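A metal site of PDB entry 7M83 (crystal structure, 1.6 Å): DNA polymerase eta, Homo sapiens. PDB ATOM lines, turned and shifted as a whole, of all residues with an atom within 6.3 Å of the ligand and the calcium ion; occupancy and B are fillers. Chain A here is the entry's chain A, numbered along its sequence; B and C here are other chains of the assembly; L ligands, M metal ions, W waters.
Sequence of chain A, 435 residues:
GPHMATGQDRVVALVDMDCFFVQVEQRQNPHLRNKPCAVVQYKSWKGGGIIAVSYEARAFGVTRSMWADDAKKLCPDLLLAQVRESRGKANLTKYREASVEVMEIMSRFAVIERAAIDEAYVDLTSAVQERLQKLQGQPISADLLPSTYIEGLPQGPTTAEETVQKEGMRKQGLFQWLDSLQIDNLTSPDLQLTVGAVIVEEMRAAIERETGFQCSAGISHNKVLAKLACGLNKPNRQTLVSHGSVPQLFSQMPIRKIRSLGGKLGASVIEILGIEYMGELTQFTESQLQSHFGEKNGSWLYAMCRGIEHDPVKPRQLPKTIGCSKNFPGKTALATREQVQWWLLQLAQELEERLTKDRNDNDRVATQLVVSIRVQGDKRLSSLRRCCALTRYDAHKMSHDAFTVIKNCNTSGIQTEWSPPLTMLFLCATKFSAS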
ATOM      1  N   ASP A  16      16.536  14.886 -17.785  1.00  0.00           N
ATOM      2  CA  ASP A  16      16.497  15.978 -16.810  1.00  0.00           C
ATOM      3  C   ASP A  16      15.213  15.817 -16.006  1.00  0.00           C
ATOM      4  O   ASP A  16      14.112  15.965 -16.560  1.00  0.00           O
ATOM      5  CB  ASP A  16      16.517  17.325 -17.557  1.00  0.00           C
ATOM      6  CG  ASP A  16      16.718  18.530 -16.660  1.00  0.00           C
ATOM      7  OD1 ASP A  16      16.447  18.441 -15.458  1.00  0.00           O
ATOM      8  OD2 ASP A  16      17.099  19.605 -17.197  1.00  0.00           O
ATOM      9  N   MET A  17      15.326  15.514 -14.705  1.00  0.00           N
ATOM     10  CA  MET A  17      14.118  15.322 -13.901  1.00  0.00           C
ATOM     11  C   MET A  17      13.323  16.619 -13.800  1.00  0.00           C
ATOM     12  O   MET A  17      13.897  17.692 -13.691  1.00  0.00           O
ATOM     13  CB  MET A  17      14.464  14.804 -12.497  1.00  0.00           C
ATOM     14  CG  MET A  17      15.380  13.584 -12.504  1.00  0.00           C
ATOM     15  SD  MET A  17      14.679  12.169 -13.426  1.00  0.00           S
ATOM     16  CE  MET A  17      13.214  11.865 -12.529  1.00  0.00           C
ATOM     17  N   ASP A  18      11.990  16.512 -13.854  1.00  0.00           N
ATOM     18  CA  ASP A  18      11.161  17.711 -13.714  1.00  0.00           C
ATOM     19  C   ASP A  18      11.102  18.138 -12.262  1.00  0.00           C
ATOM     20  O   ASP A  18      10.968  17.289 -11.369  1.00  0.00           O
ATOM     21  CB  ASP A  18       9.756  17.438 -14.239  1.00  0.00           C
ATOM     22  CG  ASP A  18       9.746  17.080 -15.732  1.00  0.00           C
ATOM     23  OD1 ASP A  18      10.584  17.600 -16.482  1.00  0.00           O
ATOM     24  OD2 ASP A  18       8.885  16.299 -16.160  1.00  0.00           O
ATOM     25  N   CYS A  19      11.199  19.453 -12.013  1.00  0.00           N
ATOM     26  CA  CYS A  19      11.131  20.078 -10.677  1.00  0.00           C
ATOM     27  C   CYS A  19      11.555  19.082  -9.585  1.00  0.00           C
ATOM     28  O   CYS A  19      10.768  18.701  -8.725  1.00  0.00           O
ATOM     29  CB  CYS A  19       9.733  20.662 -10.402  1.00  0.00           C
ATOM     30  SG  CYS A  19       8.307  19.608 -10.597  1.00  0.00           S
ATOM     31  N   PHE A  20      12.821  18.659  -9.632  1.00  0.00           N
ATOM     32  CA  PHE A  20      13.213  17.418  -8.981  1.00  0.00           C
ATOM     33  C   PHE A  20      12.957  17.384  -7.473  1.00  0.00           C
ATOM     34  O   PHE A  20      12.326  16.441  -6.981  1.00  0.00           O
ATOM     35  CB  PHE A  20      14.688  17.133  -9.264  1.00  0.00           C
ATOM     36  CG  PHE A  20      15.151  15.811  -8.699  1.00  0.00           C
ATOM     37  CD1 PHE A  20      14.436  14.642  -8.949  1.00  0.00           C
ATOM     38  CD2 PHE A  20      16.285  15.750  -7.903  1.00  0.00           C
ATOM     39  CE1 PHE A  20      14.869  13.418  -8.440  1.00  0.00           C
ATOM     40  CE2 PHE A  20      16.725  14.507  -7.384  1.00  0.00           C
ATOM     41  CZ  PHE A  20      16.001  13.352  -7.671  1.00  0.00           C
ATOM     42  N   PHE A  21      13.460  18.376  -6.729  1.00  0.00           N
ATOM     43  CA  PHE A  21      13.277  18.278  -5.274  1.00  0.00           C
ATOM     44  C   PHE A  21      11.792  18.324  -4.903  1.00  0.00           C
ATOM     45  O   PHE A  21      11.369  17.731  -3.906  1.00  0.00           O
ATOM     46  CB  PHE A  21      14.008  19.397  -4.523  1.00  0.00           C
ATOM     47  CG  PHE A  21      15.523  19.297  -4.522  1.00  0.00           C
ATOM     48  CD1 PHE A  21      16.216  18.477  -5.399  1.00  0.00           C
ATOM     49  CD2 PHE A  21      16.256  20.075  -3.640  1.00  0.00           C
ATOM     50  CE1 PHE A  21      17.614  18.440  -5.385  1.00  0.00           C
ATOM     51  CE2 PHE A  21      17.667  20.036  -3.619  1.00  0.00           C
ATOM     52  CZ  PHE A  21      18.331  19.207  -4.493  1.00  0.00           C
ATOM     53  N   VAL A  22      10.999  19.068  -5.678  1.00  0.00           N
ATOM     54  CA  VAL A  22       9.555  19.092  -5.464  1.00  0.00           C
ATOM     55  C   VAL A  22       8.980  17.695  -5.638  1.00  0.00           C
ATOM     56  O   VAL A  22       8.181  17.225  -4.820  1.00  0.00           O
ATOM     57  CB  VAL A  22       8.887  20.091  -6.410  1.00  0.00           C
ATOM     58  CG1 VAL A  22       7.363  19.871  -6.504  1.00  0.00           C
ATOM     59  CG2 VAL A  22       9.212  21.520  -6.008  1.00  0.00           C
ATOM     60  N   GLN A  41      14.800  26.269   1.829  1.00  0.00           N
ATOM     61  CA  GLN A  41      15.882  26.020   2.794  1.00  0.00           C
ATOM     62  C   GLN A  41      15.788  27.138   3.819  1.00  0.00           C
ATOM     63  O   GLN A  41      15.776  28.302   3.404  1.00  0.00           O
ATOM     64  CB  GLN A  41      17.282  26.073   2.170  1.00  0.00           C
ATOM     65  CG  GLN A  41      17.587  24.970   1.185  1.00  0.00           C
ATOM     66  CD  GLN A  41      19.014  25.060   0.718  1.00  0.00           C
ATOM     67  OE1 GLN A  41      19.500  26.117   0.341  1.00  0.00           O
ATOM     68  NE2 GLN A  41      19.692  23.926   0.744  1.00  0.00           N
ATOM     69  N   ILE A  51      14.340  26.827  -3.511  1.00  0.00           N
ATOM     70  CA  ILE A  51      15.293  26.168  -4.409  1.00  0.00           C
ATOM     71  C   ILE A  51      14.630  25.299  -5.469  1.00  0.00           C
ATOM     72  O   ILE A  51      15.312  24.883  -6.407  1.00  0.00           O
ATOM     73  CB  ILE A  51      16.366  25.375  -3.625  1.00  0.00           C
ATOM     74  CG1 ILE A  51      15.757  24.273  -2.745  1.00  0.00           C
ATOM     75  CG2 ILE A  51      17.245  26.334  -2.817  1.00  0.00           C
ATOM     76  CD1 ILE A  51      16.835  23.323  -2.180  1.00  0.00           C
ATOM     77  N   ALA A  52      13.329  25.016  -5.383  1.00  0.00           N
ATOM     78  CA  ALA A  52      12.653  24.240  -6.427  1.00  0.00           C
ATOM     79  C   ALA A  52      11.168  24.594  -6.398  1.00  0.00           C
ATOM     80  O   ALA A  52      10.621  24.887  -5.321  1.00  0.00           O
ATOM     81  CB  ALA A  52      12.843  22.721  -6.250  1.00  0.00           C
ATOM     82  N   VAL A  53      10.530  24.555  -7.580  1.00  0.00           N
ATOM     83  CA  VAL A  53       9.169  25.072  -7.756  1.00  0.00           C
ATOM     84  C   VAL A  53       8.355  24.178  -8.672  1.00  0.00           C
ATOM     85  O   VAL A  53       8.783  23.878  -9.790  1.00  0.00           O
ATOM     86  CB  VAL A  53       9.199  26.491  -8.357  1.00  0.00           C
ATOM     87  CG1 VAL A  53       7.800  27.096  -8.387  1.00  0.00           C
ATOM     88  CG2 VAL A  53      10.135  27.402  -7.582  1.00  0.00           C
ATOM     89  N   TYR A  55       5.385  23.074 -11.303  1.00  0.00           N
ATOM     90  CA  TYR A  55       4.892  23.793 -12.484  1.00  0.00           C
ATOM     91  C   TYR A  55       3.595  24.558 -12.186  1.00  0.00           C
ATOM     92  O   TYR A  55       3.380  25.670 -12.701  1.00  0.00           O
ATOM     93  CB  TYR A  55       4.749  22.817 -13.679  1.00  0.00           C
ATOM     94  CG  TYR A  55       6.107  22.524 -14.289  1.00  0.00           C
ATOM     95  CD1 TYR A  55       7.000  21.637 -13.693  1.00  0.00           C
ATOM     96  CD2 TYR A  55       6.553  23.264 -15.389  1.00  0.00           C
ATOM     97  CE1 TYR A  55       8.280  21.443 -14.227  1.00  0.00           C
ATOM     98  CE2 TYR A  55       7.805  23.060 -15.920  1.00  0.00           C
ATOM     99  CZ  TYR A  55       8.667  22.161 -15.348  1.00  0.00           C
ATOM    100  OH  TYR A  55       9.919  21.970 -15.874  1.00  0.00           O
ATOM    101  N   ARG A  58       4.848  27.704 -10.738  1.00  0.00           N
ATOM    102  CA  ARG A  58       5.471  28.565 -11.739  1.00  0.00           C
ATOM    103  C   ARG A  58       4.418  29.376 -12.492  1.00  0.00           C
ATOM    104  O   ARG A  58       4.700  30.498 -12.936  1.00  0.00           O
ATOM    105  CB  ARG A  58       6.300  27.762 -12.736  1.00  0.00           C
ATOM    106  CG  ARG A  58       7.418  27.003 -12.096  1.00  0.00           C
ATOM    107  CD  ARG A  58       8.200  26.162 -13.113  1.00  0.00           C
ATOM    108  NE  ARG A  58       9.012  25.175 -12.394  1.00  0.00           N
ATOM    109  CZ  ARG A  58      10.042  24.512 -12.896  1.00  0.00           C
ATOM    110  NH1 ARG A  58      10.439  24.717 -14.161  1.00  0.00           N
ATOM    111  NH2 ARG A  58      10.682  23.626 -12.124  1.00  0.00           N
ATOM    112  N   ARG A  64      12.856  30.143  -8.463  1.00  0.00           N
ATOM    113  CA  ARG A  64      13.981  29.871  -7.554  1.00  0.00           C
ATOM    114  C   ARG A  64      14.637  31.197  -7.181  1.00  0.00           C
ATOM    115  O   ARG A  64      14.483  32.128  -7.952  1.00  0.00           O
ATOM    116  CB  ARG A  64      15.005  28.990  -8.295  1.00  0.00           C
ATOM    117  CG  ARG A  64      16.238  28.559  -7.541  1.00  0.00           C
ATOM    118  CD  ARG A  64      17.075  27.694  -8.457  1.00  0.00           C
ATOM    119  NE  ARG A  64      16.391  26.423  -8.564  1.00  0.00           N
ATOM    120  CZ  ARG A  64      16.110  25.791  -9.688  1.00  0.00           C
ATOM    121  NH1 ARG A  64      16.470  26.294 -10.860  1.00  0.00           N
ATOM    122  NH2 ARG A  64      15.469  24.646  -9.631  1.00  0.00           N
ATOM    123  N   ILE A 117      22.724  16.593 -10.054  1.00  0.00           N
ATOM    124  CA  ILE A 117      21.954  15.735  -9.157  1.00  0.00           C
ATOM    125  C   ILE A 117      20.762  15.079  -9.846  1.00  0.00           C
ATOM    126  O   ILE A 117      20.380  13.958  -9.503  1.00  0.00           O
ATOM    127  CB  ILE A 117      21.474  16.527  -7.918  1.00  0.00           C
ATOM    128  CG1 ILE A 117      21.076  15.544  -6.820  1.00  0.00           C
ATOM    129  CG2 ILE A 117      20.344  17.485  -8.251  1.00  0.00           C
ATOM    130  CD1 ILE A 117      21.031  16.156  -5.413  1.00  0.00           C
ATOM    131  N   ASP A 118      20.231  15.706 -10.888  1.00  0.00           N
ATOM    132  CA  ASP A 118      19.038  15.179 -11.539  1.00  0.00           C
ATOM    133  C   ASP A 118      19.157  15.145 -13.049  1.00  0.00           C
ATOM    134  O   ASP A 118      18.138  15.102 -13.751  1.00  0.00           O
ATOM    135  CB  ASP A 118      17.850  16.018 -11.082  1.00  0.00           C
ATOM    136  CG  ASP A 118      17.741  17.299 -11.874  1.00  0.00           C
ATOM    137  OD1 ASP A 118      18.829  17.862 -12.210  1.00  0.00           O
ATOM    138  OD2 ASP A 118      16.610  17.753 -12.179  1.00  0.00           O
ATOM    139  N   GLU A 119      20.391  15.158 -13.569  1.00  0.00           N
ATOM    140  CA  GLU A 119      20.589  15.154 -15.017  1.00  0.00           C
ATOM    141  C   GLU A 119      21.647  14.137 -15.351  1.00  0.00           C
ATOM    142  O   GLU A 119      22.695  14.085 -14.693  1.00  0.00           O
ATOM    143  CB  GLU A 119      21.090  16.472 -15.557  1.00  0.00           C
ATOM    144  CG  GLU A 119      20.111  17.590 -15.580  1.00  0.00           C
ATOM    145  CD  GLU A 119      20.668  18.778 -16.348  1.00  0.00           C
ATOM    146  OE1 GLU A 119      21.637  18.549 -17.106  1.00  0.00           O
ATOM    147  OE2 GLU A 119      20.160  19.907 -16.206  1.00  0.00           O
ATOM    148  N   LYS A 227      20.932  18.521 -24.676  1.00  0.00           N
ATOM    149  CA  LYS A 227      20.564  19.374 -23.554  1.00  0.00           C
ATOM    150  C   LYS A 227      19.617  20.473 -24.015  1.00  0.00           C
ATOM    151  O   LYS A 227      18.598  20.742 -23.360  1.00  0.00           O
ATOM    152  CB  LYS A 227      21.823  19.951 -22.915  1.00  0.00           C
ATOM    153  CG  LYS A 227      21.601  21.013 -21.844  1.00  0.00           C
ATOM    154  CD  LYS A 227      20.862  20.462 -20.645  1.00  0.00           C
ATOM    155  CE  LYS A 227      20.875  21.447 -19.492  1.00  0.00           C
ATOM    156  NZ  LYS A 227      19.831  21.071 -18.506  1.00  0.00           N
ATOM    157  N   LYS A 234       9.663  20.660 -21.987  1.00  0.00           N
ATOM    158  CA  LYS A 234       9.548  20.214 -20.612  1.00  0.00           C
ATOM    159  C   LYS A 234       8.303  20.909 -20.035  1.00  0.00           C
ATOM    160  O   LYS A 234       7.979  22.024 -20.442  1.00  0.00           O
ATOM    161  CB  LYS A 234      10.898  20.549 -19.935  1.00  0.00           C
ATOM    162  CG  LYS A 234      11.197  20.134 -18.522  1.00  0.00           C
ATOM    163  CD  LYS A 234      12.155  21.054 -17.829  1.00  0.00           C
ATOM    164  CE  LYS A 234      13.414  20.207 -17.508  1.00  0.00           C
ATOM    165  NZ  LYS A 234      13.087  18.979 -16.636  1.00  0.00           N
ATOM    166  N   PRO A 235       7.577  20.282 -19.069  1.00  0.00           N
ATOM    167  CA  PRO A 235       7.907  18.972 -18.497  1.00  0.00           C
ATOM    168  C   PRO A 235       7.208  17.755 -19.091  1.00  0.00           C
ATOM    169  O   PRO A 235       6.238  17.844 -19.861  1.00  0.00           O
ATOM    170  CB  PRO A 235       7.397  19.114 -17.069  1.00  0.00           C
ATOM    171  CG  PRO A 235       6.096  19.928 -17.267  1.00  0.00           C
ATOM    172  CD  PRO A 235       6.400  20.872 -18.402  1.00  0.00           C
ATOM    173  P    DT B   3      20.345  38.759  -1.128  1.00  0.00           P
ATOM    174  OP1  DT B   3      21.287  39.889  -1.262  1.00  0.00           O
ATOM    175  OP2  DT B   3      18.976  38.857  -1.649  1.00  0.00           O
ATOM    176  O5'  DT B   3      21.061  37.498  -1.788  1.00  0.00           O
ATOM    177  C5'  DT B   3      20.274  36.446  -2.338  1.00  0.00           C
ATOM    178  C4'  DT B   3      20.059  35.385  -1.291  1.00  0.00           C
ATOM    179  O4'  DT B   3      19.218  34.352  -1.854  1.00  0.00           O
ATOM    180  C3'  DT B   3      21.357  34.679  -0.866  1.00  0.00           C
ATOM    181  O3'  DT B   3      21.431  34.355   0.527  1.00  0.00           O
ATOM    182  C2'  DT B   3      21.324  33.419  -1.702  1.00  0.00           C
ATOM    183  C1'  DT B   3      19.853  33.112  -1.672  1.00  0.00           C
ATOM    184  N1   DT B   3      19.438  32.205  -2.751  1.00  0.00           N
ATOM    185  C2   DT B   3      18.620  31.167  -2.404  1.00  0.00           C
ATOM    186  O2   DT B   3      18.176  31.014  -1.273  1.00  0.00           O
ATOM    187  N3   DT B   3      18.287  30.327  -3.441  1.00  0.00           N
ATOM    188  C4   DT B   3      18.713  30.411  -4.747  1.00  0.00           C
ATOM    189  O4   DT B   3      18.333  29.594  -5.569  1.00  0.00           O
ATOM    190  C5   DT B   3      19.573  31.537  -5.046  1.00  0.00           C
ATOM    191  C7   DT B   3      20.071  31.731  -6.438  1.00  0.00           C
ATOM    192  C6   DT B   3      19.892  32.364  -4.034  1.00  0.00           C
ATOM    193  P    DT B   4      22.662  33.466   1.150  1.00  0.00           P
ATOM    194  OP1  DT B   4      22.719  33.704   2.601  1.00  0.00           O
ATOM    195  OP2  DT B   4      23.854  33.651   0.284  1.00  0.00           O
ATOM    196  O5'  DT B   4      22.232  31.968   0.867  1.00  0.00           O
ATOM    197  C5'  DT B   4      21.217  31.374   1.611  1.00  0.00           C
ATOM    198  C4'  DT B   4      21.405  29.894   1.553  1.00  0.00           C
ATOM    199  O4'  DT B   4      21.106  29.490   0.195  1.00  0.00           O
ATOM    200  C3'  DT B   4      22.825  29.392   1.824  1.00  0.00           C
ATOM    201  O3'  DT B   4      22.697  28.206   2.589  1.00  0.00           O
ATOM    202  C2'  DT B   4      23.393  29.147   0.430  1.00  0.00           C
ATOM    203  C1'  DT B   4      22.152  28.689  -0.301  1.00  0.00           C
ATOM    204  N1   DT B   4      22.201  28.896  -1.785  1.00  0.00           N
ATOM    205  C2   DT B   4      21.635  27.950  -2.589  1.00  0.00           C
ATOM    206  O2   DT B   4      21.193  26.919  -2.162  1.00  0.00           O
ATOM    207  N3   DT B   4      21.676  28.229  -3.926  1.00  0.00           N
ATOM    208  C4   DT B   4      22.172  29.360  -4.530  1.00  0.00           C
ATOM    209  O4   DT B   4      22.145  29.510  -5.749  1.00  0.00           O
ATOM    210  C5   DT B   4      22.709  30.358  -3.624  1.00  0.00           C
ATOM    211  C7   DT B   4      23.291  31.636  -4.178  1.00  0.00           C
ATOM    212  C6   DT B   4      22.689  30.080  -2.311  1.00  0.00           C
ATOM    213  P    DT B   5      23.969  27.373   3.086  1.00  0.00           P
ATOM    214  OP1  DT B   5      23.597  26.798   4.384  1.00  0.00           O
ATOM    215  OP2  DT B   5      25.178  28.211   2.921  1.00  0.00           O
ATOM    216  O5'  DT B   5      24.034  26.167   2.034  1.00  0.00           O
ATOM    217  C5'  DT B   5      23.022  25.177   2.064  1.00  0.00           C
ATOM    218  C4'  DT B   5      23.297  24.131   1.008  1.00  0.00           C
ATOM    219  O4'  DT B   5      23.181  24.734  -0.303  1.00  0.00           O
ATOM    220  C3'  DT B   5      24.709  23.528   1.072  1.00  0.00           C
ATOM    221  O3'  DT B   5      24.629  22.120   0.771  1.00  0.00           O
ATOM    222  C2'  DT B   5      25.444  24.287  -0.036  1.00  0.00           C
ATOM    223  C1'  DT B   5      24.316  24.381  -1.054  1.00  0.00           C
ATOM    224  N1   DT B   5      24.531  25.365  -2.117  1.00  0.00           N
ATOM    225  C2   DT B   5      24.052  25.063  -3.363  1.00  0.00           C
ATOM    226  O2   DT B   5      23.461  24.014  -3.611  1.00  0.00           O
ATOM    227  N3   DT B   5      24.277  26.003  -4.313  1.00  0.00           N
ATOM    228  C4   DT B   5      24.915  27.219  -4.144  1.00  0.00           C
ATOM    229  O4   DT B   5      25.060  28.011  -5.065  1.00  0.00           O
ATOM    230  C5   DT B   5      25.380  27.496  -2.793  1.00  0.00           C
ATOM    231  C7   DT B   5      26.096  28.786  -2.483  1.00  0.00           C
ATOM    232  C6   DT B   5      25.166  26.551  -1.850  1.00  0.00           C
ATOM    233  P    DA C   8      22.670  22.903 -16.186  1.00  0.00           P
ATOM    234  OP1  DA C   8      22.551  21.542 -16.743  1.00  0.00           O
ATOM    235  OP2  DA C   8      21.796  23.992 -16.679  1.00  0.00           O
ATOM    236  O5'  DA C   8      22.496  22.825 -14.606  1.00  0.00           O
ATOM    237  C5'  DA C   8      21.312  22.337 -14.052  1.00  0.00           C
ATOM    238  C4'  DA C   8      21.666  21.376 -12.953  1.00  0.00           C
ATOM    239  O4'  DA C   8      22.731  21.960 -12.137  1.00  0.00           O
ATOM    240  C3'  DA C   8      20.550  21.005 -11.999  1.00  0.00           C
ATOM    241  O3'  DA C   8      20.730  19.700 -11.495  1.00  0.00           O
ATOM    242  C2'  DA C   8      20.707  22.057 -10.903  1.00  0.00           C
ATOM    243  C1'  DA C   8      22.226  22.208 -10.826  1.00  0.00           C
ATOM    244  N9   DA C   8      22.672  23.530 -10.402  1.00  0.00           N
ATOM    245  C8   DA C   8      22.957  24.607 -11.198  1.00  0.00           C
ATOM    246  N7   DA C   8      23.330  25.669 -10.534  1.00  0.00           N
ATOM    247  C5   DA C   8      23.310  25.254  -9.199  1.00  0.00           C
ATOM    248  C6   DA C   8      23.624  25.918  -8.005  1.00  0.00           C
ATOM    249  N6   DA C   8      24.050  27.176  -7.942  1.00  0.00           N
ATOM    250  N1   DA C   8      23.493  25.222  -6.862  1.00  0.00           N
ATOM    251  C2   DA C   8      23.068  23.953  -6.916  1.00  0.00           C
ATOM    252  N3   DA C   8      22.753  23.225  -7.987  1.00  0.00           N
ATOM    253  C4   DA C   8      22.896  23.945  -9.112  1.00  0.00           C
HETATM  254  P1  LIG L   1      13.037  21.801 -14.083  1.00  0.00           P
HETATM  255  O1  LIG L   1      12.984  23.105 -14.818  1.00  0.00           O
HETATM  256  O2  LIG L   1      11.791  21.036 -14.300  1.00  0.00           O
HETATM  257  O3  LIG L   1      14.220  20.966 -14.455  1.00  0.00           O
HETATM  258  P2  LIG L   1      14.256  21.667 -11.488  1.00  0.00           P
HETATM  259  O4  LIG L   1      14.562  20.195 -11.606  1.00  0.00           O
HETATM  260  O5  LIG L   1      13.764  22.005 -10.136  1.00  0.00           O
HETATM  261  O6  LIG L   1      13.172  22.107 -12.555  1.00  0.00           O
HETATM  262  P3  LIG L   1      17.012  22.102 -12.024  1.00  0.00           P
HETATM  263  O7  LIG L   1      17.749  23.322 -12.465  1.00  0.00           O
HETATM  264  O8  LIG L   1      17.095  21.015 -13.032  1.00  0.00           O
HETATM  265  O9  LIG L   1      15.547  22.518 -11.783  1.00  0.00           O
HETATM  266  O10 LIG L   1      17.594  21.637 -10.638  1.00  0.00           O
HETATM  267  C1  LIG L   1      17.448  20.359 -10.144  1.00  0.00           C
HETATM  268  C2  LIG L   1      17.398  20.407  -8.635  1.00  0.00           C
HETATM  269  O11 LIG L   1      18.623  21.005  -8.147  1.00  0.00           O
HETATM  270  C3  LIG L   1      16.296  21.373  -8.210  1.00  0.00           C
HETATM  271  O12 LIG L   1      15.088  20.667  -7.994  1.00  0.00           O
HETATM  272  C4  LIG L   1      16.840  21.873  -6.884  1.00  0.00           C
HETATM  273  C5  LIG L   1      18.289  21.905  -7.086  1.00  0.00           C
HETATM  274  N1  LIG L   1      18.795  23.244  -7.464  1.00  0.00           N
HETATM  275  C6  LIG L   1      18.763  23.794  -8.680  1.00  0.00           C
HETATM  276  N2  LIG L   1      19.303  25.009  -8.661  1.00  0.00           N
HETATM  277  C7  LIG L   1      19.711  25.247  -7.386  1.00  0.00           C
HETATM  278  C8  LIG L   1      20.325  26.313  -6.755  1.00  0.00           C
HETATM  279  N3  LIG L   1      20.646  27.403  -7.448  1.00  0.00           N
HETATM  280  N4  LIG L   1      20.580  26.218  -5.482  1.00  0.00           N
HETATM  281  C9  LIG L   1      20.245  25.116  -4.815  1.00  0.00           C
HETATM  282  N5  LIG L   1      19.669  24.078  -5.324  1.00  0.00           N
HETATM  283  C10 LIG L   1      19.384  24.122  -6.623  1.00  0.00           C
HETATM  284 CA    CA M   1      15.553  19.257 -13.562  1.00  0.00          CA
HETATM  285  O   HOH W   1      13.952  25.506 -13.815  1.00  0.00           O
HETATM  286  O   HOH W   2      12.326  24.209  -9.691  1.00  0.00           O
HETATM  287  O   HOH W   3      19.642  25.323 -11.567  1.00  0.00           O
HETATM  288  O   HOH W   4      20.420  21.872  -3.660  1.00  0.00           O
HETATM  289  O   HOH W   5      21.517  20.803  -7.633  1.00  0.00           O
HETATM  290  O   HOH W   6      20.308  28.568 -10.178  1.00  0.00           O
HETATM  291  O   HOH W   7      15.181  23.305 -16.562  1.00  0.00           O
HETATM  292  O   HOH W   8      16.468  25.474 -13.875  1.00  0.00           O
HETATM  293  O   HOH W   9      17.527  21.885 -15.649  1.00  0.00           O
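The backbone NH of Phe 20 is in hydrogen-bond range of an oxygen (O12) of the ligand (3.4 Å).
OH of Tyr 55 is in hydrogen-bond range of O2 of the ligand, 2.6 Å away.
A nitrogen (N3) of the ligand lies close to N6 of DA 8 of chain C, 3.4 Å away.
The backbone NH of Cys 19 lies within hydrogen-bond range of an oxygen (O2) of the ligand, 2.8 Å away.
O4 of DT 4 of chain B lies within hydrogen-bond range of N3 of the ligand.
The backbone NH of Phe 21 is in hydrogen-bond range of an oxygen (O12) of the ligand (3.1 Å).
NH1 of Arg 58 lies within salt-bridge range of O1 of the ligand (3.1 Å).
O5 of the ligand is in salt-bridge range of NH2 of Arg 64, 3.2 Å away.
NZ of Lys 234 lies within salt-bridge range of O2 of the ligand (3.4 Å).
O2 of DT 4 of chain B lies close to the side-chain amide oxygen (OE1) of Gln 41 (3.1 Å).
O3' of DA 8 of chain C lies close to the side-chain carboxylate of Asp 118 (2.7 Å).
NH1 of Arg 58 lies within hydrogen-bond range of OH of Tyr 55, at 3.3 Å.
The backbone carbonyl oxygen (O) of Ile 51 is in hydrogen-bond range of the guanidinium group (NE) of Arg 64, 2.9 Å away.
The backbone carbonyl oxygen (O) of Met 17 sits close to the side-chain amino group (NZ) of Lys 234, at 3.3 Å.
NE of Arg 58 is in hydrogen-bond range of O of Val 53 (2.9 Å).
The side-chain amino group (NZ) of Lys 234 is in salt-bridge range of the side-chain carboxylate (OD1) of Asp 18.
OD2 of Asp 16 is in salt-bridge range of NZ of Lys 227.
Asp 18 touches the ligand (CA to O2, 3.4 Å).
O of Ile 51 touches C4 of the ligand (3.4 Å).
Ala 52 touches the ligand.
Ile 117 touches the ligand.
DT 3 of chain B touches the ligand (O4 to N3, 3.7 Å).
O2 of DT 5 of chain B touches C9 of the ligand (3.6 Å).
Hydrophobic or aromatic side chains within 4 Å of the ligand: Phe 20, Phe 21, Ile 51, Ala 52, Tyr 55 and Ile 117.
18 residues have an atom within 4 Å of the ligand: Asp 16, Met 17, Asp 18, Cys 19, Phe 20, Phe 21, Ile 51, Ala 52, Tyr 55, Arg 58, Arg 64, Ile 117, Asp 118, Lys 234, DT 3 of chain B, DT 4 of chain B, DT 5 of chain B and DA 8 of chain C.
Along chain A the residues within 4 Å of the ligand span positions 16 to 234.
The nearest printed residue that does not touch the ligand is Glu 119 (4.5 Å).
Residues that only touch the calcium ion: Lys 234 (3.95 Å).
Of the 24 residues printed, 4 come within 4 Å of the calcium ion.
Along chain A the residues within 4 Å of the calcium ion span positions 16 to 234.
The nearest printed residue that does not touch the calcium ion is Asp 18 (4.5 Å).
The calcium ion is bound by the side-chain carboxylate of Asp 16, the backbone carbonyl oxygen of Met 17, the side-chain carboxylate of Asp 118, an oxygen (O3) of the ligand, an oxygen (O4) of the ligand and an oxygen (O8) of the ligand.
The calcium ion has six donor atoms within binding distance.
Water W9 bridges OD2 of Asp 16 (2.8 Å) and OE2 of Glu 119 (3.3 Å).
Water W8 bridges O7 of the ligand (2.9 Å) and NH1 of Arg 64 (3.1 Å).
Water W3 lies within hydrogen-bond range of O7 of the ligand and NH1 of Arg 64.
Water W5 bridges N3 of DA 8 of chain C and an oxygen (O11) of the ligand.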
